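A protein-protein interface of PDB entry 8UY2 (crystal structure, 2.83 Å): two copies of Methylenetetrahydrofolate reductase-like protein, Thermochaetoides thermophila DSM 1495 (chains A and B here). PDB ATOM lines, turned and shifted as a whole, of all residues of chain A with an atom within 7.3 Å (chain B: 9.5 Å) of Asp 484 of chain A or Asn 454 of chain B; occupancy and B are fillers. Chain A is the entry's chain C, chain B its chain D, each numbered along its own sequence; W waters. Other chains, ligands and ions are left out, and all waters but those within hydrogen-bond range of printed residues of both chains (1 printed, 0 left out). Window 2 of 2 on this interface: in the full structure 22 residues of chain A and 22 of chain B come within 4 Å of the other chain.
Printed residues of chain B that touch a printed residue of chain A: Asn 454, Tyr 456, Val 512, Phe 513, Pro 514, Gly 515 and Lys 516. Hydrophobic or aromatic side chains of chain B that line the printed part of chain A: Tyr 456, Val 512 and Pro 514. Along chain B the printed residues that touch a printed residue of chain A span positions 454 to 516. Hydrophobic or aromatic side chains of chain A that line the printed part of chain B: Phe 574. Along chain A the printed residues that touch a printed residue of chain B span positions 460 to 574. Among the printed residues, 12 pairs touch across the chains.
OD1 of Asp 573 of chain A lies within hydrogen-bond range of OH of Tyr 456 of chain B (3.3 Å). The side-chain amide oxygen of Asn 572 of chain A lies within hydrogen-bond range of the backbone NH of Gly 515 of chain B, at 3.1 Å. The backbone carbonyl oxygen (O) of Lys 516 of chain B lies close to the side-chain amide oxygen (OD1) of Asn 506 of chain A, 3.4 Å away.
ND2 of Asn 506 of chain A is in hydrogen-bond range of OD1 of Asn 572 of chain A (3.0 Å). The side-chain amino group (NZ) of Lys 460 of chain A lies within hydrogen-bond range of the side-chain amide oxygen (OD1) of Asn 572 of chain A (3.2 Å). The side-chain amide nitrogen of Asn 572 of chain A is in hydrogen-bond range of the backbone carbonyl oxygen of Asp 484 of chain A (3.0 Å). The side-chain hydroxyl of Thr 486 of chain A lies within hydrogen-bond range of the side-chain amide nitrogen of Asn 572 of chain A, at 2.8 Å. The side-chain carboxylate of Asp 484 of chain A lies within hydrogen-bond range of the backbone NH of Asp 573 of chain A. The backbone NH (N) of Asp 573 of chain A sits at hydrogen-bond distance from the side-chain amide oxygen (OD1) of Asn 571 of chain A (3.1 Å).
Water W1 lies within hydrogen-bond range of O of Asn 572 of chain A and O of Val 512 of chain B.
CE of Lys 460 of chain A touches CG1 of Val 512 of chain B, 3.9 Å away. O of Phe 513 of chain B touches NZ of Lys 460 of chain A (3.8 Å). Lys 516 of chain B touches Lys 460 of chain A. OD1 of Asp 484 of chain A touches CB of Asn 454 of chain B (3.7 Å). CG of Pro 514 of chain B touches OD1 of Asp 484 of chain A, 3.3 Å away. CA of Gly 515 of chain B touches CG of Asn 506 of chain A, 3.5 Å away. Asn 572 of chain A touches Pro 514 of chain B. CE1 of Phe 574 of chain A touches CD2 of Tyr 456 of chain B, 3.8 Å away. Phe 574 of chain A touches Val 512 of chain B (CE1 to CG1, 3.6 Å).
No position is printed for both chains. Of the 12 pairs that touch across the chains among the printed residues, none has its exchanged pair printed and touching as well.
Pro 483 of chain A touches none of the printed residues of chain B. Of chain B, only Asn 454 and Pro 514 come within 4 Å of Asp 484 of chain A. No residue of chain B comes within 4 Å of Leu 485 of chain A. Thr 486 of chain A touches none of the printed residues of chain B. Of chain B, only Pro 514 and Gly 515 come within 4 Å of Asn 572 of chain A. Of the printed residues of chain B, Asp 573 of chain A touches Tyr 456 (3.3 Å). Asn 454 of chain B touches just one residue of chain A: Asp 484. Printed residues of chain A within 4 Å of Tyr 456 of chain B: Asp 573 and Phe 574. Of the printed residues of chain A, Phe 513 of chain B touches Lys 460 (3.8 Å). Of the printed residues of chain A, Gly 515 of chain B touches Asn 506 (3.5 Å) and Asn 572 (3.1 Å). The nearest residue of chain B that does not touch Asp 484 of chain A is Ser 453 of chain B (5.7 Å). The nearest residue of chain A that does not touch Asn 454 of chain B is Asn 572 of chain A (5.9 Å). The nearest printed residue of chain A that does not touch Phe 513 of chain B is Asn 506 of chain A (4.6 Å).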
ATOM      1  N   LYS A 460     -17.588  36.646  25.345  1.00  0.00           N
ATOM      2  CA  LYS A 460     -17.721  35.271  25.788  1.00  0.00           C
ATOM      3  C   LYS A 460     -18.548  35.281  27.072  1.00  0.00           C
ATOM      4  O   LYS A 460     -18.277  36.103  27.959  1.00  0.00           O
ATOM      5  CB  LYS A 460     -16.360  34.617  26.031  1.00  0.00           C
ATOM      6  CG  LYS A 460     -15.576  34.340  24.772  1.00  0.00           C
ATOM      7  CD  LYS A 460     -14.129  33.989  25.070  1.00  0.00           C
ATOM      8  CE  LYS A 460     -13.290  33.716  23.854  1.00  0.00           C
ATOM      9  NZ  LYS A 460     -11.851  33.724  24.169  1.00  0.00           N
ATOM     10  N   ILE A 479     -17.483  20.259  33.669  1.00  0.00           N
ATOM     11  CA  ILE A 479     -16.755  21.247  32.879  1.00  0.00           C
ATOM     12  C   ILE A 479     -15.711  20.542  32.013  1.00  0.00           C
ATOM     13  O   ILE A 479     -15.638  20.820  30.811  1.00  0.00           O
ATOM     14  CB  ILE A 479     -16.094  22.313  33.764  1.00  0.00           C
ATOM     15  CG1 ILE A 479     -17.109  23.175  34.499  1.00  0.00           C
ATOM     16  CG2 ILE A 479     -15.143  23.192  32.937  1.00  0.00           C
ATOM     17  CD1 ILE A 479     -16.525  23.900  35.707  1.00  0.00           C
ATOM     18  N   GLU A 480     -14.914  19.657  32.641  1.00  0.00           N
ATOM     19  CA  GLU A 480     -13.863  18.912  31.951  1.00  0.00           C
ATOM     20  C   GLU A 480     -14.367  18.155  30.711  1.00  0.00           C
ATOM     21  O   GLU A 480     -13.637  18.084  29.717  1.00  0.00           O
ATOM     22  CB  GLU A 480     -13.192  17.938  32.913  1.00  0.00           C
ATOM     23  CG  GLU A 480     -12.321  18.624  33.964  1.00  0.00           C
ATOM     24  CD  GLU A 480     -11.711  17.721  35.029  1.00  0.00           C
ATOM     25  OE1 GLU A 480     -11.998  16.494  35.107  1.00  0.00           O
ATOM     26  OE2 GLU A 480     -10.937  18.297  35.835  1.00  0.00           O
ATOM     27  N   SER A 481     -15.620  17.662  30.766  1.00  0.00           N
ATOM     28  CA  SER A 481     -16.228  16.976  29.636  1.00  0.00           C
ATOM     29  C   SER A 481     -16.521  17.894  28.442  1.00  0.00           C
ATOM     30  O   SER A 481     -16.668  17.381  27.335  1.00  0.00           O
ATOM     31  CB  SER A 481     -17.462  16.240  30.071  1.00  0.00           C
ATOM     32  OG  SER A 481     -18.545  17.119  30.332  1.00  0.00           O
ATOM     33  N   HIS A 482     -16.655  19.218  28.669  1.00  0.00           N
ATOM     34  CA  HIS A 482     -16.903  20.193  27.610  1.00  0.00           C
ATOM     35  C   HIS A 482     -15.633  20.997  27.325  1.00  0.00           C
ATOM     36  O   HIS A 482     -15.376  21.978  28.023  1.00  0.00           O
ATOM     37  CB  HIS A 482     -18.080  21.094  27.962  1.00  0.00           C
ATOM     38  CG  HIS A 482     -19.395  20.396  27.960  1.00  0.00           C
ATOM     39  ND1 HIS A 482     -19.700  19.368  28.824  1.00  0.00           N
ATOM     40  CD2 HIS A 482     -20.471  20.547  27.165  1.00  0.00           C
ATOM     41  CE1 HIS A 482     -20.939  18.959  28.589  1.00  0.00           C
ATOM     42  NE2 HIS A 482     -21.419  19.651  27.579  1.00  0.00           N
ATOM     43  N   PRO A 483     -14.850  20.647  26.276  1.00  0.00           N
ATOM     44  CA  PRO A 483     -13.497  21.187  26.106  1.00  0.00           C
ATOM     45  C   PRO A 483     -13.375  22.668  25.750  1.00  0.00           C
ATOM     46  O   PRO A 483     -12.301  23.233  25.924  1.00  0.00           O
ATOM     47  CB  PRO A 483     -12.915  20.273  25.009  1.00  0.00           C
ATOM     48  CG  PRO A 483     -14.106  19.906  24.159  1.00  0.00           C
ATOM     49  CD  PRO A 483     -15.267  19.825  25.130  1.00  0.00           C
ATOM     50  N   ASP A 484     -14.481  23.293  25.304  1.00  0.00           N
ATOM     51  CA  ASP A 484     -14.487  24.698  24.913  1.00  0.00           C
ATOM     52  C   ASP A 484     -14.750  25.626  26.095  1.00  0.00           C
ATOM     53  O   ASP A 484     -14.881  26.841  25.906  1.00  0.00           O
ATOM     54  CB  ASP A 484     -15.490  24.905  23.787  1.00  0.00           C
ATOM     55  CG  ASP A 484     -15.112  25.951  22.752  1.00  0.00           C
ATOM     56  OD1 ASP A 484     -13.971  25.917  22.296  1.00  0.00           O
ATOM     57  OD2 ASP A 484     -15.966  26.754  22.376  1.00  0.00           O
ATOM     58  N   LEU A 485     -14.864  25.063  27.312  1.00  0.00           N
ATOM     59  CA  LEU A 485     -14.967  25.818  28.542  1.00  0.00           C
ATOM     60  C   LEU A 485     -13.603  25.923  29.193  1.00  0.00           C
ATOM     61  O   LEU A 485     -12.939  24.914  29.321  1.00  0.00           O
ATOM     62  CB  LEU A 485     -15.960  25.155  29.487  1.00  0.00           C
ATOM     63  CG  LEU A 485     -17.332  24.814  28.896  1.00  0.00           C
ATOM     64  CD1 LEU A 485     -18.236  24.362  30.009  1.00  0.00           C
ATOM     65  CD2 LEU A 485     -17.968  25.975  28.156  1.00  0.00           C
ATOM     66  N   THR A 486     -13.212  27.125  29.617  1.00  0.00           N
ATOM     67  CA  THR A 486     -12.033  27.328  30.443  1.00  0.00           C
ATOM     68  C   THR A 486     -12.525  27.564  31.859  1.00  0.00           C
ATOM     69  O   THR A 486     -13.393  28.412  32.036  1.00  0.00           O
ATOM     70  CB  THR A 486     -11.222  28.524  29.954  1.00  0.00           C
ATOM     71  OG1 THR A 486     -11.040  28.420  28.544  1.00  0.00           O
ATOM     72  CG2 THR A 486      -9.874  28.632  30.661  1.00  0.00           C
ATOM     73  N   ASN A 499      -8.215  23.979  33.760  1.00  0.00           N
ATOM     74  CA  ASN A 499      -7.959  23.192  32.550  1.00  0.00           C
ATOM     75  C   ASN A 499      -7.124  23.956  31.527  1.00  0.00           C
ATOM     76  O   ASN A 499      -6.819  23.393  30.480  1.00  0.00           O
ATOM     77  CB  ASN A 499      -9.261  22.743  31.920  1.00  0.00           C
ATOM     78  CG  ASN A 499     -10.178  23.891  31.566  1.00  0.00           C
ATOM     79  OD1 ASN A 499      -9.862  25.074  31.803  1.00  0.00           O
ATOM     80  ND2 ASN A 499     -11.350  23.551  31.075  1.00  0.00           N
ATOM     81  N   ASN A 506      -7.102  35.125  28.800  1.00  0.00           N
ATOM     82  CA  ASN A 506      -8.217  34.774  27.935  1.00  0.00           C
ATOM     83  C   ASN A 506      -9.107  36.001  27.790  1.00  0.00           C
ATOM     84  O   ASN A 506      -9.696  36.431  28.778  1.00  0.00           O
ATOM     85  CB  ASN A 506      -8.986  33.581  28.487  1.00  0.00           C
ATOM     86  CG  ASN A 506     -10.087  33.060  27.577  1.00  0.00           C
ATOM     87  OD1 ASN A 506     -10.203  33.440  26.402  1.00  0.00           O
ATOM     88  ND2 ASN A 506     -10.864  32.118  28.091  1.00  0.00           N
ATOM     89  N   VAL A 570     -15.643  30.130  31.759  1.00  0.00           N
ATOM     90  CA  VAL A 570     -15.806  30.900  30.542  1.00  0.00           C
ATOM     91  C   VAL A 570     -16.194  29.925  29.444  1.00  0.00           C
ATOM     92  O   VAL A 570     -15.535  28.903  29.277  1.00  0.00           O
ATOM     93  CB  VAL A 570     -14.511  31.654  30.220  1.00  0.00           C
ATOM     94  CG1 VAL A 570     -14.529  32.255  28.821  1.00  0.00           C
ATOM     95  CG2 VAL A 570     -14.223  32.738  31.252  1.00  0.00           C
ATOM     96  N   ASN A 571     -17.213  30.303  28.665  1.00  0.00           N
ATOM     97  CA  ASN A 571     -17.588  29.574  27.468  1.00  0.00           C
ATOM     98  C   ASN A 571     -16.962  30.302  26.294  1.00  0.00           C
ATOM     99  O   ASN A 571     -17.478  31.333  25.897  1.00  0.00           O
ATOM    100  CB  ASN A 571     -19.097  29.464  27.321  1.00  0.00           C
ATOM    101  CG  ASN A 571     -19.507  28.748  26.052  1.00  0.00           C
ATOM    102  OD1 ASN A 571     -18.695  28.124  25.346  1.00  0.00           O
ATOM    103  ND2 ASN A 571     -20.784  28.838  25.735  1.00  0.00           N
ATOM    104  N   ASN A 572     -15.931  29.698  25.704  1.00  0.00           N
ATOM    105  CA  ASN A 572     -15.179  30.352  24.636  1.00  0.00           C
ATOM    106  C   ASN A 572     -16.005  30.475  23.353  1.00  0.00           C
ATOM    107  O   ASN A 572     -15.685  31.331  22.525  1.00  0.00           O
ATOM    108  CB  ASN A 572     -13.821  29.697  24.414  1.00  0.00           C
ATOM    109  CG  ASN A 572     -12.895  29.918  25.600  1.00  0.00           C
ATOM    110  OD1 ASN A 572     -12.251  30.969  25.725  1.00  0.00           O
ATOM    111  ND2 ASN A 572     -12.805  28.930  26.481  1.00  0.00           N
ATOM    112  N   ASP A 573     -17.059  29.655  23.194  1.00  0.00           N
ATOM    113  CA  ASP A 573     -17.974  29.837  22.092  1.00  0.00           C
ATOM    114  C   ASP A 573     -18.990  30.949  22.402  1.00  0.00           C
ATOM    115  O   ASP A 573     -20.017  30.696  23.003  1.00  0.00           O
ATOM    116  CB  ASP A 573     -18.639  28.558  21.626  1.00  0.00           C
ATOM    117  CG  ASP A 573     -19.370  28.694  20.296  1.00  0.00           C
ATOM    118  OD1 ASP A 573     -19.354  29.805  19.705  1.00  0.00           O
ATOM    119  OD2 ASP A 573     -19.936  27.676  19.858  1.00  0.00           O
ATOM    120  N   PHE A 574     -18.737  32.118  21.842  1.00  0.00           N
ATOM    121  CA  PHE A 574     -19.524  33.322  22.077  1.00  0.00           C
ATOM    122  C   PHE A 574     -20.739  33.377  21.145  1.00  0.00           C
ATOM    123  O   PHE A 574     -21.506  34.346  21.217  1.00  0.00           O
ATOM    124  CB  PHE A 574     -18.651  34.576  21.919  1.00  0.00           C
ATOM    125  CG  PHE A 574     -17.924  34.690  20.599  1.00  0.00           C
ATOM    126  CD1 PHE A 574     -16.684  34.065  20.454  1.00  0.00           C
ATOM    127  CD2 PHE A 574     -18.492  35.332  19.503  1.00  0.00           C
ATOM    128  CE1 PHE A 574     -15.998  34.115  19.244  1.00  0.00           C
ATOM    129  CE2 PHE A 574     -17.790  35.411  18.301  1.00  0.00           C
ATOM    130  CZ  PHE A 574     -16.545  34.779  18.165  1.00  0.00           C
ATOM    131  N   GLN A 576     -22.860  30.981  21.644  1.00  0.00           N
ATOM    132  CA  GLN A 576     -23.763  30.277  22.539  1.00  0.00           C
ATOM    133  C   GLN A 576     -24.001  31.056  23.834  1.00  0.00           C
ATOM    134  O   GLN A 576     -23.063  31.257  24.625  1.00  0.00           O
ATOM    135  CB  GLN A 576     -23.209  28.907  22.921  1.00  0.00           C
ATOM    136  CG  GLN A 576     -22.712  28.055  21.761  1.00  0.00           C
ATOM    137  CD  GLN A 576     -22.071  26.768  22.236  1.00  0.00           C
ATOM    138  OE1 GLN A 576     -21.256  26.741  23.159  1.00  0.00           O
ATOM    139  NE2 GLN A 576     -22.450  25.652  21.642  1.00  0.00           N
ATOM    140  N   ASP B 249      -2.129  26.322  11.038  1.00  0.00           N
ATOM    141  CA  ASP B 249      -1.791  26.626  12.416  1.00  0.00           C
ATOM    142  C   ASP B 249      -0.275  26.646  12.575  1.00  0.00           C
ATOM    143  O   ASP B 249       0.341  25.588  12.662  1.00  0.00           O
ATOM    144  CB  ASP B 249      -2.434  25.665  13.399  1.00  0.00           C
ATOM    145  CG  ASP B 249      -2.170  25.969  14.872  1.00  0.00           C
ATOM    146  OD1 ASP B 249      -1.461  26.953  15.162  1.00  0.00           O
ATOM    147  OD2 ASP B 249      -2.654  25.216  15.730  1.00  0.00           O
ATOM    148  N   ALA B 441     -15.849  33.155  10.262  1.00  0.00           N
ATOM    149  CA  ALA B 441     -15.663  31.806   9.769  1.00  0.00           C
ATOM    150  C   ALA B 441     -15.060  30.953  10.885  1.00  0.00           C
ATOM    151  O   ALA B 441     -14.225  31.439  11.648  1.00  0.00           O
ATOM    152  CB  ALA B 441     -14.772  31.815   8.566  1.00  0.00           C
ATOM    153  N   LYS B 442     -15.466  29.678  10.965  1.00  0.00           N
ATOM    154  CA  LYS B 442     -14.780  28.728  11.821  1.00  0.00           C
ATOM    155  C   LYS B 442     -13.314  28.670  11.397  1.00  0.00           C
ATOM    156  O   LYS B 442     -13.002  28.804  10.214  1.00  0.00           O
ATOM    157  CB  LYS B 442     -15.389  27.332  11.775  1.00  0.00           C
ATOM    158  CG  LYS B 442     -16.823  27.224  12.274  1.00  0.00           C
ATOM    159  CD  LYS B 442     -17.288  25.781  12.437  1.00  0.00           C
ATOM    160  CE  LYS B 442     -17.315  24.975  11.159  1.00  0.00           C
ATOM    161  NZ  LYS B 442     -17.658  23.578  11.397  1.00  0.00           N
ATOM    162  N   SER B 443     -12.424  28.514  12.381  1.00  0.00           N
ATOM    163  CA  SER B 443     -10.988  28.547  12.163  1.00  0.00           C
ATOM    164  C   SER B 443     -10.469  27.368  11.335  1.00  0.00           C
ATOM    165  O   SER B 443      -9.314  27.397  10.936  1.00  0.00           O
ATOM    166  CB  SER B 443     -10.261  28.644  13.476  1.00  0.00           C
ATOM    167  OG  SER B 443     -10.482  27.517  14.311  1.00  0.00           O
ATOM    168  N   ASN B 444     -11.295  26.324  11.127  1.00  0.00           N
ATOM    169  CA  ASN B 444     -10.975  25.214  10.252  1.00  0.00           C
ATOM    170  C   ASN B 444     -11.530  25.386   8.841  1.00  0.00           C
ATOM    171  O   ASN B 444     -11.463  24.441   8.062  1.00  0.00           O
ATOM    172  CB  ASN B 444     -11.426  23.907  10.892  1.00  0.00           C
ATOM    173  CG  ASN B 444     -12.926  23.712  10.940  1.00  0.00           C
ATOM    174  OD1 ASN B 444     -13.705  24.584  10.522  1.00  0.00           O
ATOM    175  ND2 ASN B 444     -13.349  22.587  11.485  1.00  0.00           N
ATOM    176  N   HIS B 445     -12.156  26.533   8.541  1.00  0.00           N
ATOM    177  CA  HIS B 445     -12.687  26.792   7.226  1.00  0.00           C
ATOM    178  C   HIS B 445     -11.605  26.570   6.164  1.00  0.00           C
ATOM    179  O   HIS B 445     -10.497  27.074   6.317  1.00  0.00           O
ATOM    180  CB  HIS B 445     -13.255  28.207   7.103  1.00  0.00           C
ATOM    181  CG  HIS B 445     -14.019  28.478   5.858  1.00  0.00           C
ATOM    182  ND1 HIS B 445     -13.438  28.540   4.617  1.00  0.00           N
ATOM    183  CD2 HIS B 445     -15.332  28.698   5.672  1.00  0.00           C
ATOM    184  CE1 HIS B 445     -14.373  28.796   3.721  1.00  0.00           C
ATOM    185  NE2 HIS B 445     -15.535  28.896   4.337  1.00  0.00           N
ATOM    186  N   TRP B 450      -7.581  29.733   9.839  1.00  0.00           N
ATOM    187  CA  TRP B 450      -6.192  29.684  10.290  1.00  0.00           C
ATOM    188  C   TRP B 450      -6.133  29.551  11.804  1.00  0.00           C
ATOM    189  O   TRP B 450      -7.144  29.686  12.488  1.00  0.00           O
ATOM    190  CB  TRP B 450      -5.418  30.928   9.817  1.00  0.00           C
ATOM    191  CG  TRP B 450      -6.054  32.223  10.228  1.00  0.00           C
ATOM    192  CD1 TRP B 450      -7.010  32.912   9.550  1.00  0.00           C
ATOM    193  CD2 TRP B 450      -5.783  32.965  11.422  1.00  0.00           C
ATOM    194  NE1 TRP B 450      -7.341  34.046  10.235  1.00  0.00           N
ATOM    195  CE2 TRP B 450      -6.609  34.111  11.383  1.00  0.00           C
ATOM    196  CE3 TRP B 450      -4.925  32.781  12.512  1.00  0.00           C
ATOM    197  CZ2 TRP B 450      -6.605  35.063  12.406  1.00  0.00           C
ATOM    198  CZ3 TRP B 450      -4.904  33.733  13.518  1.00  0.00           C
ATOM    199  CH2 TRP B 450      -5.745  34.856  13.470  1.00  0.00           C
ATOM    200  N   GLY B 451      -4.942  29.266  12.319  1.00  0.00           N
ATOM    201  CA  GLY B 451      -4.735  29.125  13.750  1.00  0.00           C
ATOM    202  C   GLY B 451      -5.281  27.806  14.285  1.00  0.00           C
ATOM    203  O   GLY B 451      -5.638  26.916  13.504  1.00  0.00           O
ATOM    204  N   PRO B 452      -5.384  27.639  15.623  1.00  0.00           N
ATOM    205  CA  PRO B 452      -5.926  26.412  16.212  1.00  0.00           C
ATOM    206  C   PRO B 452      -7.409  26.199  15.929  1.00  0.00           C
ATOM    207  O   PRO B 452      -8.041  27.039  15.298  1.00  0.00           O
ATOM    208  CB  PRO B 452      -5.632  26.580  17.708  1.00  0.00           C
ATOM    209  CG  PRO B 452      -5.575  28.060  17.919  1.00  0.00           C
ATOM    210  CD  PRO B 452      -5.000  28.625  16.651  1.00  0.00           C
ATOM    211  N   SER B 453      -7.935  25.065  16.385  1.00  0.00           N
ATOM    212  CA  SER B 453      -9.309  24.681  16.089  1.00  0.00           C
ATOM    213  C   SER B 453     -10.269  25.167  17.171  1.00  0.00           C
ATOM    214  O   SER B 453      -9.879  25.501  18.290  1.00  0.00           O
ATOM    215  CB  SER B 453      -9.406  23.197  15.841  1.00  0.00           C
ATOM    216  OG  SER B 453      -9.106  22.925  14.481  1.00  0.00           O
ATOM    217  N   ASN B 454     -11.557  25.152  16.803  1.00  0.00           N
ATOM    218  CA  ASN B 454     -12.642  25.659  17.632  1.00  0.00           C
ATOM    219  C   ASN B 454     -12.459  27.152  17.888  1.00  0.00           C
ATOM    220  O   ASN B 454     -12.764  27.626  18.973  1.00  0.00           O
ATOM    221  CB  ASN B 454     -12.831  24.862  18.921  1.00  0.00           C
ATOM    222  CG  ASN B 454     -13.090  23.404  18.659  1.00  0.00           C
ATOM    223  OD1 ASN B 454     -12.217  22.562  18.885  1.00  0.00           O
ATOM    224  ND2 ASN B 454     -14.299  23.078  18.221  1.00  0.00           N
ATOM    225  N   GLY B 455     -11.967  27.877  16.865  1.00  0.00           N
ATOM    226  CA  GLY B 455     -11.908  29.324  16.864  1.00  0.00           C
ATOM    227  C   GLY B 455     -12.784  29.943  15.784  1.00  0.00           C
ATOM    228  O   GLY B 455     -13.370  29.240  14.958  1.00  0.00           O
ATOM    229  N   TYR B 456     -12.874  31.279  15.802  1.00  0.00           N
ATOM    230  CA  TYR B 456     -13.551  32.043  14.760  1.00  0.00           C
ATOM    231  C   TYR B 456     -12.602  33.119  14.252  1.00  0.00           C
ATOM    232  O   TYR B 456     -11.882  33.726  15.035  1.00  0.00           O
ATOM    233  CB  TYR B 456     -14.896  32.578  15.253  1.00  0.00           C
ATOM    234  CG  TYR B 456     -15.820  31.467  15.697  1.00  0.00           C
ATOM    235  CD1 TYR B 456     -16.587  30.763  14.766  1.00  0.00           C
ATOM    236  CD2 TYR B 456     -15.881  31.072  17.039  1.00  0.00           C
ATOM    237  CE1 TYR B 456     -17.430  29.722  15.155  1.00  0.00           C
ATOM    238  CE2 TYR B 456     -16.733  30.046  17.447  1.00  0.00           C
ATOM    239  CZ  TYR B 456     -17.512  29.372  16.504  1.00  0.00           C
ATOM    240  OH  TYR B 456     -18.333  28.358  16.889  1.00  0.00           O
ATOM    241  N   VAL B 457     -12.631  33.383  12.946  1.00  0.00           N
ATOM    242  CA  VAL B 457     -11.704  34.318  12.328  1.00  0.00           C
ATOM    243  C   VAL B 457     -12.494  35.360  11.553  1.00  0.00           C
ATOM    244  O   VAL B 457     -13.566  35.084  11.016  1.00  0.00           O
ATOM    245  CB  VAL B 457     -10.689  33.608  11.426  1.00  0.00           C
ATOM    246  CG1 VAL B 457      -9.858  32.611  12.220  1.00  0.00           C
ATOM    247  CG2 VAL B 457     -11.339  32.927  10.213  1.00  0.00           C
ATOM    248  N   GLY B 511      -8.501  36.819  15.043  1.00  0.00           N
ATOM    249  CA  GLY B 511      -8.971  35.484  15.367  1.00  0.00           C
ATOM    250  C   GLY B 511      -9.248  35.330  16.855  1.00  0.00           C
ATOM    251  O   GLY B 511      -8.452  35.795  17.681  1.00  0.00           O
ATOM    252  N   VAL B 512     -10.345  34.628  17.171  1.00  0.00           N
ATOM    253  CA  VAL B 512     -10.791  34.391  18.533  1.00  0.00           C
ATOM    254  C   VAL B 512     -10.639  32.897  18.777  1.00  0.00           C
ATOM    255  O   VAL B 512     -11.362  32.121  18.157  1.00  0.00           O
ATOM    256  CB  VAL B 512     -12.230  34.866  18.745  1.00  0.00           C
ATOM    257  CG1 VAL B 512     -12.626  34.810  20.217  1.00  0.00           C
ATOM    258  CG2 VAL B 512     -12.419  36.277  18.200  1.00  0.00           C
ATOM    259  N   PHE B 513      -9.725  32.522  19.690  1.00  0.00           N
ATOM    260  CA  PHE B 513      -9.416  31.135  19.951  1.00  0.00           C
ATOM    261  C   PHE B 513      -9.583  30.817  21.432  1.00  0.00           C
ATOM    262  O   PHE B 513      -9.299  31.683  22.271  1.00  0.00           O
ATOM    263  CB  PHE B 513      -8.013  30.816  19.488  1.00  0.00           C
ATOM    264  CG  PHE B 513      -7.792  31.125  18.028  1.00  0.00           C
ATOM    265  CD1 PHE B 513      -8.246  30.256  17.035  1.00  0.00           C
ATOM    266  CD2 PHE B 513      -7.118  32.284  17.659  1.00  0.00           C
ATOM    267  CE1 PHE B 513      -8.024  30.537  15.693  1.00  0.00           C
ATOM    268  CE2 PHE B 513      -6.897  32.566  16.313  1.00  0.00           C
ATOM    269  CZ  PHE B 513      -7.356  31.690  15.327  1.00  0.00           C
ATOM    270  N   PRO B 514      -9.993  29.571  21.793  1.00  0.00           N
ATOM    271  CA  PRO B 514     -10.205  29.192  23.187  1.00  0.00           C
ATOM    272  C   PRO B 514      -9.029  29.483  24.110  1.00  0.00           C
ATOM    273  O   PRO B 514      -7.916  29.171  23.726  1.00  0.00           O
ATOM    274  CB  PRO B 514     -10.468  27.702  23.108  1.00  0.00           C
ATOM    275  CG  PRO B 514     -11.098  27.521  21.777  1.00  0.00           C
ATOM    276  CD  PRO B 514     -10.349  28.457  20.896  1.00  0.00           C
ATOM    277  N   GLY B 515      -9.292  30.181  25.221  1.00  0.00           N
ATOM    278  CA  GLY B 515      -8.298  30.382  26.258  1.00  0.00           C
ATOM    279  C   GLY B 515      -7.213  31.380  25.877  1.00  0.00           C
ATOM    280  O   GLY B 515      -6.181  31.387  26.547  1.00  0.00           O
ATOM    281  N   LYS B 516      -7.416  32.179  24.811  1.00  0.00           N
ATOM    282  CA  LYS B 516      -6.385  33.067  24.300  1.00  0.00           C
ATOM    283  C   LYS B 516      -6.882  34.504  24.178  1.00  0.00           C
ATOM    284  O   LYS B 516      -8.091  34.760  24.138  1.00  0.00           O
ATOM    285  CB  LYS B 516      -5.831  32.481  23.007  1.00  0.00           C
ATOM    286  CG  LYS B 516      -4.894  31.299  23.321  1.00  0.00           C
ATOM    287  CD  LYS B 516      -4.310  30.532  22.132  1.00  0.00           C
ATOM    288  CE  LYS B 516      -3.398  31.299  21.205  1.00  0.00           C
ATOM    289  NZ  LYS B 516      -2.937  30.524  20.036  1.00  0.00           N
HETATM  290  O   HOH W   1     -13.360  31.040  20.724  1.00  0.00           O
